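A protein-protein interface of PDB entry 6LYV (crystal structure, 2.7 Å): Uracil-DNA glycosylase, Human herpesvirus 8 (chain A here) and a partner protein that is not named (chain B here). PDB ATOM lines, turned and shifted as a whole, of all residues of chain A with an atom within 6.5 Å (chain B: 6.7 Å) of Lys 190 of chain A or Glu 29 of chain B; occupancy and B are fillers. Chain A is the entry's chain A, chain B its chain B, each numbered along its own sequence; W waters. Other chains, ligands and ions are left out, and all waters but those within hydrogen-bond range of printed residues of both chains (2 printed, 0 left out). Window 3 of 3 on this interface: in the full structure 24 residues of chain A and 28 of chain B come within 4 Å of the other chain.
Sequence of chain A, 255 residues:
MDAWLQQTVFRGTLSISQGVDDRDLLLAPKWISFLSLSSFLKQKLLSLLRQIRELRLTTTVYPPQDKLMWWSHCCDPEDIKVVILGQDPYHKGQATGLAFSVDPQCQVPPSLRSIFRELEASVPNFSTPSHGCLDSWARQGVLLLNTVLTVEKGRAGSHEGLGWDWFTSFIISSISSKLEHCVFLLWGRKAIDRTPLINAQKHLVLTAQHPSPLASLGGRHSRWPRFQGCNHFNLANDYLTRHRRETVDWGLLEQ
The backbone NH of Arg 189 of chain A is in hydrogen-bond range of the side-chain carboxylate of Glu 30 of chain B (3.0 Å).
The side-chain amide nitrogen (NE2) of Gln 87 of chain A sits at hydrogen-bond distance from the backbone carbonyl oxygen (O) of Glu 29 of chain B, at 2.9 Å.
O of Gln 87 of chain A sits at hydrogen-bond distance from N of Thr 147 of chain A.
The backbone carbonyl oxygen (O) of Glu 30 of chain B sits at hydrogen-bond distance from the backbone NH (N) of Leu 51 of chain B (2.7 Å).
The backbone carbonyl oxygen of Lys 190 of chain A lies within hydrogen-bond range of the guanidinium group of Arg 194 of chain A, 2.8 Å away.
OG1 of Thr 53 of chain B sits at hydrogen-bond distance from O of Ile 28 of chain B (2.5 Å).
The guanidinium group of Arg 189 of chain A is in salt-bridge range of the side-chain carboxylate of Asp 193 of chain A, 2.8 Å away.
The side-chain amide nitrogen of Gln 52 of chain B is in hydrogen-bond range of the side-chain carboxylate of Glu 29 of chain B, at 2.9 Å.
Gln 87 of chain A touches Ile 28 of chain B (NE2 to CG2, 3.6 Å).
OE1 of Glu 30 of chain B touches CA of Gly 188 of chain A (3.1 Å).
CG of Arg 189 of chain A touches CG2 of Ile 31 of chain B, 3.9 Å away.
Ile 50 of chain B touches Arg 189 of chain A (CD1 to CG, 3.7 Å).
Lys 190 of chain A touches Glu 29 of chain B.
Ile 28 of chain B touches His 210 of chain A (CD1 to NE2, 3.4 Å).
His 210 of chain A touches Glu 30 of chain B.
CZ3 of Trp 224 of chain A touches OE2 of Glu 30 of chain B, 3.7 Å away.
Trp 224 of chain A touches Ile 31 of chain B (CH2 to CD1, 3.5 Å).
Of chain B, only Glu 29 (3.2 Å) comes within 4 Å of Lys 190 of chain A.
Glu 29 of chain B touches just these residues of chain A: Gln 87 and Lys 190.
Printed residues of chain B within 4 Å of Gln 87 of chain A: Ile 28 (3.6 Å) and Glu 29 (2.9 Å).
Of the printed residues of chain A, Ile 31 of chain B touches Arg 189 and Trp 224.
Of the printed residues of chain B, Gly 188 of chain A touches Glu 30.
Printed residues of chain B within 4 Å of His 210 of chain A: Ile 28 and Glu 30.
Ile 192 of chain A touches none of the printed residues of chain B.
The nearest residue of chain A that does not touch Glu 29 of chain B is His 210 of chain A (5.0 Å).
The nearest printed residue of chain A that does not touch Glu 30 of chain B is Lys 190 of chain A (4.7 Å).
Of the 9 printed residues of chain B, 5 touch a printed residue of chain A.
Printed residues of chain B that touch a printed residue of chain A: Ile 28, Glu 29, Glu 30, Ile 31 and Ile 50.
Hydrophobic or aromatic side chains of chain B within 4 Å of the printed part of chain A: Ile 28, Ile 31 and Ile 50.
Of the 17 printed residues of chain A, 6 touch a printed residue of chain B.
Among the printed residues, 11 pairs touch across the chains.
Among the printed residues, no Asp or Glu carboxylate lies within 4 Å of a Lys or Arg side-chain nitrogen of the other chain.
Water W2 lies within hydrogen-bond range of O of Asp 88 of chain A (2.7 Å) and O of Ser 27 of chain B (3.0 Å).
Water W1 bridges OE2 of Glu 29 of chain B (2.9 Å) and NZ of Lys 190 of chain A (3.1 Å).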
ATOM      1  N   LEU A  85     -14.971   9.243  19.161  1.00  0.00           N
ATOM      2  CA  LEU A  85     -13.808   8.368  19.237  1.00  0.00           C
ATOM      3  C   LEU A  85     -13.275   8.303  20.662  1.00  0.00           C
ATOM      4  O   LEU A  85     -13.097   9.336  21.315  1.00  0.00           O
ATOM      5  CB  LEU A  85     -12.706   8.854  18.297  1.00  0.00           C
ATOM      6  CG  LEU A  85     -13.006   8.811  16.801  1.00  0.00           C
ATOM      7  CD1 LEU A  85     -11.742   9.091  16.013  1.00  0.00           C
ATOM      8  CD2 LEU A  85     -13.597   7.471  16.411  1.00  0.00           C
ATOM      9  N   GLY A  86     -13.025   7.084  21.140  1.00  0.00           N
ATOM     10  CA  GLY A  86     -12.279   6.872  22.359  1.00  0.00           C
ATOM     11  C   GLY A  86     -10.857   6.411  22.069  1.00  0.00           C
ATOM     12  O   GLY A  86     -10.415   6.319  20.927  1.00  0.00           O
ATOM     13  N   GLN A  87     -10.136   6.105  23.144  1.00  0.00           N
ATOM     14  CA  GLN A  87      -8.782   5.588  22.998  1.00  0.00           C
ATOM     15  C   GLN A  87      -8.783   4.072  23.163  1.00  0.00           C
ATOM     16  O   GLN A  87      -9.265   3.350  22.283  1.00  0.00           O
ATOM     17  CB  GLN A  87      -7.843   6.256  24.002  1.00  0.00           C
ATOM     18  CG  GLN A  87      -7.723   7.762  23.809  1.00  0.00           C
ATOM     19  CD  GLN A  87      -6.812   8.408  24.830  1.00  0.00           C
ATOM     20  OE1 GLN A  87      -5.965   7.746  25.430  1.00  0.00           O
ATOM     21  NE2 GLN A  87      -6.990   9.704  25.045  1.00  0.00           N
ATOM     22  N   ASP A  88      -8.255   3.580  24.275  1.00  0.00           N
ATOM     23  CA  ASP A  88      -8.322   2.167  24.610  1.00  0.00           C
ATOM     24  C   ASP A  88      -9.357   1.945  25.709  1.00  0.00           C
ATOM     25  O   ASP A  88      -9.764   2.895  26.386  1.00  0.00           O
ATOM     26  CB  ASP A  88      -6.947   1.641  25.051  1.00  0.00           C
ATOM     27  CG  ASP A  88      -6.456   2.280  26.324  1.00  0.00           C
ATOM     28  OD1 ASP A  88      -6.799   3.455  26.584  1.00  0.00           O
ATOM     29  OD2 ASP A  88      -5.727   1.595  27.072  1.00  0.00           O
ATOM     30  N   THR A 147     -10.431   3.605  19.657  1.00  0.00           N
ATOM     31  CA  THR A 147      -9.463   3.402  18.583  1.00  0.00           C
ATOM     32  C   THR A 147      -8.646   2.135  18.792  1.00  0.00           C
ATOM     33  O   THR A 147      -8.152   1.552  17.821  1.00  0.00           O
ATOM     34  CB  THR A 147      -8.550   4.622  18.449  1.00  0.00           C
ATOM     35  OG1 THR A 147      -8.003   4.960  19.730  1.00  0.00           O
ATOM     36  CG2 THR A 147      -9.325   5.809  17.892  1.00  0.00           C
ATOM     37  N   GLY A 157      -3.111   1.057  27.829  1.00  0.00           N
ATOM     38  CA  GLY A 157      -2.353   1.117  26.597  1.00  0.00           C
ATOM     39  C   GLY A 157      -1.494  -0.092  26.321  1.00  0.00           C
ATOM     40  O   GLY A 157      -0.607  -0.025  25.472  1.00  0.00           O
ATOM     41  N   GLU A 160      -1.354  -1.208  22.588  1.00  0.00           N
ATOM     42  CA  GLU A 160      -1.068  -0.161  21.613  1.00  0.00           C
ATOM     43  C   GLU A 160      -0.511  -0.729  20.314  1.00  0.00           C
ATOM     44  O   GLU A 160      -0.808  -0.211  19.232  1.00  0.00           O
ATOM     45  CB  GLU A 160      -0.051   0.816  22.201  1.00  0.00           C
ATOM     46  CG  GLU A 160       0.323   1.969  21.292  1.00  0.00           C
ATOM     47  CD  GLU A 160       1.473   2.809  21.838  1.00  0.00           C
ATOM     48  OE1 GLU A 160       2.007   2.478  22.920  1.00  0.00           O
ATOM     49  OE2 GLU A 160       1.851   3.796  21.171  1.00  0.00           O
ATOM     50  N   TRP A 187     -12.092  14.486  20.457  1.00  0.00           N
ATOM     51  CA  TRP A 187     -11.689  15.077  21.729  1.00  0.00           C
ATOM     52  C   TRP A 187     -10.315  14.550  22.114  1.00  0.00           C
ATOM     53  O   TRP A 187     -10.142  13.341  22.306  1.00  0.00           O
ATOM     54  CB  TRP A 187     -12.699  14.755  22.831  1.00  0.00           C
ATOM     55  CG  TRP A 187     -14.107  15.120  22.504  1.00  0.00           C
ATOM     56  CD1 TRP A 187     -14.524  16.114  21.670  1.00  0.00           C
ATOM     57  CD2 TRP A 187     -15.293  14.487  22.999  1.00  0.00           C
ATOM     58  NE1 TRP A 187     -15.897  16.144  21.618  1.00  0.00           N
ATOM     59  CE2 TRP A 187     -16.393  15.155  22.426  1.00  0.00           C
ATOM     60  CE3 TRP A 187     -15.531  13.424  23.874  1.00  0.00           C
ATOM     61  CZ2 TRP A 187     -17.709  14.793  22.700  1.00  0.00           C
ATOM     62  CZ3 TRP A 187     -16.838  13.070  24.146  1.00  0.00           C
ATOM     63  CH2 TRP A 187     -17.909  13.751  23.560  1.00  0.00           C
ATOM     64  N   GLY A 188      -9.351  15.450  22.242  1.00  0.00           N
ATOM     65  CA  GLY A 188      -8.018  15.063  22.650  1.00  0.00           C
ATOM     66  C   GLY A 188      -7.119  14.707  21.477  1.00  0.00           C
ATOM     67  O   GLY A 188      -7.567  14.423  20.370  1.00  0.00           O
ATOM     68  N   ARG A 189      -5.813  14.725  21.753  1.00  0.00           N
ATOM     69  CA  ARG A 189      -4.811  14.516  20.711  1.00  0.00           C
ATOM     70  C   ARG A 189      -5.016  13.189  19.988  1.00  0.00           C
ATOM     71  O   ARG A 189      -4.942  13.127  18.754  1.00  0.00           O
ATOM     72  CB  ARG A 189      -3.418  14.581  21.339  1.00  0.00           C
ATOM     73  CG  ARG A 189      -2.250  14.290  20.411  1.00  0.00           C
ATOM     74  CD  ARG A 189      -2.087  15.371  19.358  1.00  0.00           C
ATOM     75  NE  ARG A 189      -2.818  15.085  18.133  1.00  0.00           N
ATOM     76  CZ  ARG A 189      -2.857  15.906  17.088  1.00  0.00           C
ATOM     77  NH1 ARG A 189      -3.537  15.572  15.998  1.00  0.00           N
ATOM     78  NH2 ARG A 189      -2.218  17.067  17.140  1.00  0.00           N
ATOM     79  N   LYS A 190      -5.291  12.116  20.737  1.00  0.00           N
ATOM     80  CA  LYS A 190      -5.414  10.800  20.118  1.00  0.00           C
ATOM     81  C   LYS A 190      -6.598  10.741  19.165  1.00  0.00           C
ATOM     82  O   LYS A 190      -6.483  10.197  18.060  1.00  0.00           O
ATOM     83  CB  LYS A 190      -5.536   9.715  21.188  1.00  0.00           C
ATOM     84  CG  LYS A 190      -4.227   9.398  21.895  1.00  0.00           C
ATOM     85  CD  LYS A 190      -3.150   8.982  20.907  1.00  0.00           C
ATOM     86  CE  LYS A 190      -1.865   8.601  21.622  1.00  0.00           C
ATOM     87  NZ  LYS A 190      -0.704   8.531  20.691  1.00  0.00           N
ATOM     88  N   ALA A 191      -7.739  11.309  19.562  1.00  0.00           N
ATOM     89  CA  ALA A 191      -8.903  11.297  18.680  1.00  0.00           C
ATOM     90  C   ALA A 191      -8.697  12.219  17.487  1.00  0.00           C
ATOM     91  O   ALA A 191      -9.089  11.888  16.362  1.00  0.00           O
ATOM     92  CB  ALA A 191     -10.159  11.694  19.456  1.00  0.00           C
ATOM     93  N   ILE A 192      -8.065  13.373  17.706  1.00  0.00           N
ATOM     94  CA  ILE A 192      -7.849  14.312  16.617  1.00  0.00           C
ATOM     95  C   ILE A 192      -6.838  13.771  15.615  1.00  0.00           C
ATOM     96  O   ILE A 192      -6.851  14.169  14.447  1.00  0.00           O
ATOM     97  CB  ILE A 192      -7.433  15.672  17.207  1.00  0.00           C
ATOM     98  CG1 ILE A 192      -8.561  16.203  18.093  1.00  0.00           C
ATOM     99  CG2 ILE A 192      -7.139  16.677  16.111  1.00  0.00           C
ATOM    100  CD1 ILE A 192      -8.124  17.249  19.083  1.00  0.00           C
ATOM    101  N   ASP A 193      -5.977  12.839  16.036  1.00  0.00           N
ATOM    102  CA  ASP A 193      -5.074  12.182  15.095  1.00  0.00           C
ATOM    103  C   ASP A 193      -5.815  11.492  13.955  1.00  0.00           C
ATOM    104  O   ASP A 193      -5.218  11.249  12.898  1.00  0.00           O
ATOM    105  CB  ASP A 193      -4.205  11.161  15.827  1.00  0.00           C
ATOM    106  CG  ASP A 193      -3.047  11.800  16.556  1.00  0.00           C
ATOM    107  OD1 ASP A 193      -2.613  12.895  16.136  1.00  0.00           O
ATOM    108  OD2 ASP A 193      -2.571  11.202  17.545  1.00  0.00           O
ATOM    109  N   ARG A 194      -7.093  11.165  14.143  1.00  0.00           N
ATOM    110  CA  ARG A 194      -7.900  10.522  13.114  1.00  0.00           C
ATOM    111  C   ARG A 194      -8.613  11.520  12.210  1.00  0.00           C
ATOM    112  O   ARG A 194      -9.440  11.106  11.390  1.00  0.00           O
ATOM    113  CB  ARG A 194      -8.930   9.586  13.754  1.00  0.00           C
ATOM    114  CG  ARG A 194      -8.402   8.212  14.129  1.00  0.00           C
ATOM    115  CD  ARG A 194      -7.506   8.247  15.348  1.00  0.00           C
ATOM    116  NE  ARG A 194      -6.954   6.928  15.636  1.00  0.00           N
ATOM    117  CZ  ARG A 194      -5.971   6.705  16.501  1.00  0.00           C
ATOM    118  NH1 ARG A 194      -5.526   5.471  16.695  1.00  0.00           N
ATOM    119  NH2 ARG A 194      -5.436   7.715  17.173  1.00  0.00           N
ATOM    120  N   HIS A 210      -9.757  17.073  25.278  1.00  0.00           N
ATOM    121  CA  HIS A 210     -10.301  15.878  25.896  1.00  0.00           C
ATOM    122  C   HIS A 210     -11.199  16.259  27.072  1.00  0.00           C
ATOM    123  O   HIS A 210     -10.884  17.194  27.818  1.00  0.00           O
ATOM    124  CB  HIS A 210      -9.170  14.964  26.366  1.00  0.00           C
ATOM    125  CG  HIS A 210      -9.608  13.563  26.652  1.00  0.00           C
ATOM    126  ND1 HIS A 210     -10.186  13.195  27.847  1.00  0.00           N
ATOM    127  CD2 HIS A 210      -9.557  12.441  25.897  1.00  0.00           C
ATOM    128  CE1 HIS A 210     -10.469  11.905  27.818  1.00  0.00           C
ATOM    129  NE2 HIS A 210     -10.097  11.423  26.646  1.00  0.00           N
ATOM    130  N   TRP A 224      -6.856  23.384  20.988  1.00  0.00           N
ATOM    131  CA  TRP A 224      -8.260  23.167  20.698  1.00  0.00           C
ATOM    132  C   TRP A 224      -9.137  23.824  21.751  1.00  0.00           C
ATOM    133  O   TRP A 224      -8.684  24.089  22.871  1.00  0.00           O
ATOM    134  CB  TRP A 224      -8.538  21.659  20.621  1.00  0.00           C
ATOM    135  CG  TRP A 224      -7.532  20.961  19.763  1.00  0.00           C
ATOM    136  CD1 TRP A 224      -7.394  21.073  18.412  1.00  0.00           C
ATOM    137  CD2 TRP A 224      -6.500  20.068  20.199  1.00  0.00           C
ATOM    138  NE1 TRP A 224      -6.350  20.295  17.975  1.00  0.00           N
ATOM    139  CE2 TRP A 224      -5.783  19.670  19.055  1.00  0.00           C
ATOM    140  CE3 TRP A 224      -6.120  19.559  21.445  1.00  0.00           C
ATOM    141  CZ2 TRP A 224      -4.710  18.783  19.118  1.00  0.00           C
ATOM    142  CZ3 TRP A 224      -5.050  18.680  21.505  1.00  0.00           C
ATOM    143  CH2 TRP A 224      -4.360  18.302  20.348  1.00  0.00           C
ATOM    144  N   SER B  27      -7.723   5.964  32.778  1.00  0.00           N
ATOM    145  CA  SER B  27      -6.451   6.272  32.140  1.00  0.00           C
ATOM    146  C   SER B  27      -6.691   6.868  30.760  1.00  0.00           C
ATOM    147  O   SER B  27      -7.446   6.310  29.958  1.00  0.00           O
ATOM    148  CB  SER B  27      -5.573   5.026  32.036  1.00  0.00           C
ATOM    149  OG  SER B  27      -4.281   5.365  31.565  1.00  0.00           O
ATOM    150  N   ILE B  28      -6.025   7.986  30.483  1.00  0.00           N
ATOM    151  CA  ILE B  28      -6.213   8.752  29.256  1.00  0.00           C
ATOM    152  C   ILE B  28      -4.855   9.269  28.809  1.00  0.00           C
ATOM    153  O   ILE B  28      -4.057   9.732  29.631  1.00  0.00           O
ATOM    154  CB  ILE B  28      -7.211   9.915  29.471  1.00  0.00           C
ATOM    155  CG1 ILE B  28      -8.640   9.382  29.552  1.00  0.00           C
ATOM    156  CG2 ILE B  28      -7.096  10.962  28.376  1.00  0.00           C
ATOM    157  CD1 ILE B  28      -9.069   8.613  28.321  1.00  0.00           C
ATOM    158  N   GLU B  29      -4.580   9.164  27.512  1.00  0.00           N
ATOM    159  CA  GLU B  29      -3.376   9.725  26.912  1.00  0.00           C
ATOM    160  C   GLU B  29      -3.685  11.101  26.335  1.00  0.00           C
ATOM    161  O   GLU B  29      -4.680  11.272  25.621  1.00  0.00           O
ATOM    162  CB  GLU B  29      -2.830   8.801  25.822  1.00  0.00           C
ATOM    163  CG  GLU B  29      -2.014   7.629  26.341  1.00  0.00           C
ATOM    164  CD  GLU B  29      -1.409   6.805  25.216  1.00  0.00           C
ATOM    165  OE1 GLU B  29      -2.068   6.665  24.164  1.00  0.00           O
ATOM    166  OE2 GLU B  29      -0.274   6.306  25.378  1.00  0.00           O
ATOM    167  N   GLU B  30      -2.844  12.080  26.655  1.00  0.00           N
ATOM    168  CA  GLU B  30      -3.040  13.439  26.169  1.00  0.00           C
ATOM    169  C   GLU B  30      -1.692  14.150  26.161  1.00  0.00           C
ATOM    170  O   GLU B  30      -0.811  13.836  26.967  1.00  0.00           O
ATOM    171  CB  GLU B  30      -4.059  14.191  27.038  1.00  0.00           C
ATOM    172  CG  GLU B  30      -4.527  15.514  26.457  1.00  0.00           C
ATOM    173  CD  GLU B  30      -4.994  15.377  25.027  1.00  0.00           C
ATOM    174  OE1 GLU B  30      -5.837  14.496  24.764  1.00  0.00           O
ATOM    175  OE2 GLU B  30      -4.502  16.130  24.161  1.00  0.00           O
ATOM    176  N   ILE B  31      -1.531  15.097  25.232  1.00  0.00           N
ATOM    177  CA  ILE B  31      -0.284  15.855  25.164  1.00  0.00           C
ATOM    178  C   ILE B  31      -0.134  16.715  26.412  1.00  0.00           C
ATOM    179  O   ILE B  31      -1.114  17.226  26.973  1.00  0.00           O
ATOM    180  CB  ILE B  31      -0.206  16.721  23.894  1.00  0.00           C
ATOM    181  CG1 ILE B  31      -1.578  17.284  23.541  1.00  0.00           C
ATOM    182  CG2 ILE B  31       0.385  15.938  22.735  1.00  0.00           C
ATOM    183  CD1 ILE B  31      -1.550  18.195  22.351  1.00  0.00           C
ATOM    184  N   ILE B  50       3.170  13.001  24.455  1.00  0.00           N
ATOM    185  CA  ILE B  50       1.992  12.346  25.010  1.00  0.00           C
ATOM    186  C   ILE B  50       2.275  11.897  26.436  1.00  0.00           C
ATOM    187  O   ILE B  50       3.261  11.197  26.700  1.00  0.00           O
ATOM    188  CB  ILE B  50       1.566  11.158  24.132  1.00  0.00           C
ATOM    189  CG1 ILE B  50       0.983  11.650  22.807  1.00  0.00           C
ATOM    190  CG2 ILE B  50       0.554  10.297  24.865  1.00  0.00           C
ATOM    191  CD1 ILE B  50      -0.370  12.327  22.949  1.00  0.00           C
ATOM    192  N   LEU B  51       1.410  12.301  27.362  1.00  0.00           N
ATOM    193  CA  LEU B  51       1.461  11.837  28.739  1.00  0.00           C
ATOM    194  C   LEU B  51       0.422  10.745  28.950  1.00  0.00           C
ATOM    195  O   LEU B  51      -0.721  10.870  28.500  1.00  0.00           O
ATOM    196  CB  LEU B  51       1.197  12.984  29.718  1.00  0.00           C
ATOM    197  CG  LEU B  51       2.143  14.182  29.698  1.00  0.00           C
ATOM    198  CD1 LEU B  51       1.753  15.172  30.785  1.00  0.00           C
ATOM    199  CD2 LEU B  51       3.586  13.741  29.857  1.00  0.00           C
ATOM    200  N   GLN B  52       0.825   9.670  29.626  1.00  0.00           N
ATOM    201  CA  GLN B  52      -0.110   8.650  30.096  1.00  0.00           C
ATOM    202  C   GLN B  52      -0.637   9.099  31.452  1.00  0.00           C
ATOM    203  O   GLN B  52       0.118   9.151  32.430  1.00  0.00           O
ATOM    204  CB  GLN B  52       0.547   7.273  30.191  1.00  0.00           C
ATOM    205  CG  GLN B  52       0.856   6.619  28.852  1.00  0.00           C
ATOM    206  CD  GLN B  52       2.046   7.237  28.143  1.00  0.00           C
ATOM    207  OE1 GLN B  52       3.069   7.533  28.761  1.00  0.00           O
ATOM    208  NE2 GLN B  52       1.912   7.447  26.838  1.00  0.00           N
ATOM    209  N   THR B  53      -1.921   9.436  31.511  1.00  0.00           N
ATOM    210  CA  THR B  53      -2.519  10.026  32.700  1.00  0.00           C
ATOM    211  C   THR B  53      -3.420   9.017  33.392  1.00  0.00           C
ATOM    212  O   THR B  53      -4.082   8.208  32.734  1.00  0.00           O
ATOM    213  CB  THR B  53      -3.333  11.265  32.352  1.00  0.00           C
ATOM    214  OG1 THR B  53      -4.585  10.860  31.788  1.00  0.00           O
ATOM    215  CG2 THR B  53      -2.580  12.124  31.343  1.00  0.00           C
HETATM  216  O   HOH W   1       0.927   7.371  23.008  1.00  0.00           O
HETATM  217  O   HOH W   2      -9.061   5.127  27.671  1.00  0.00           O
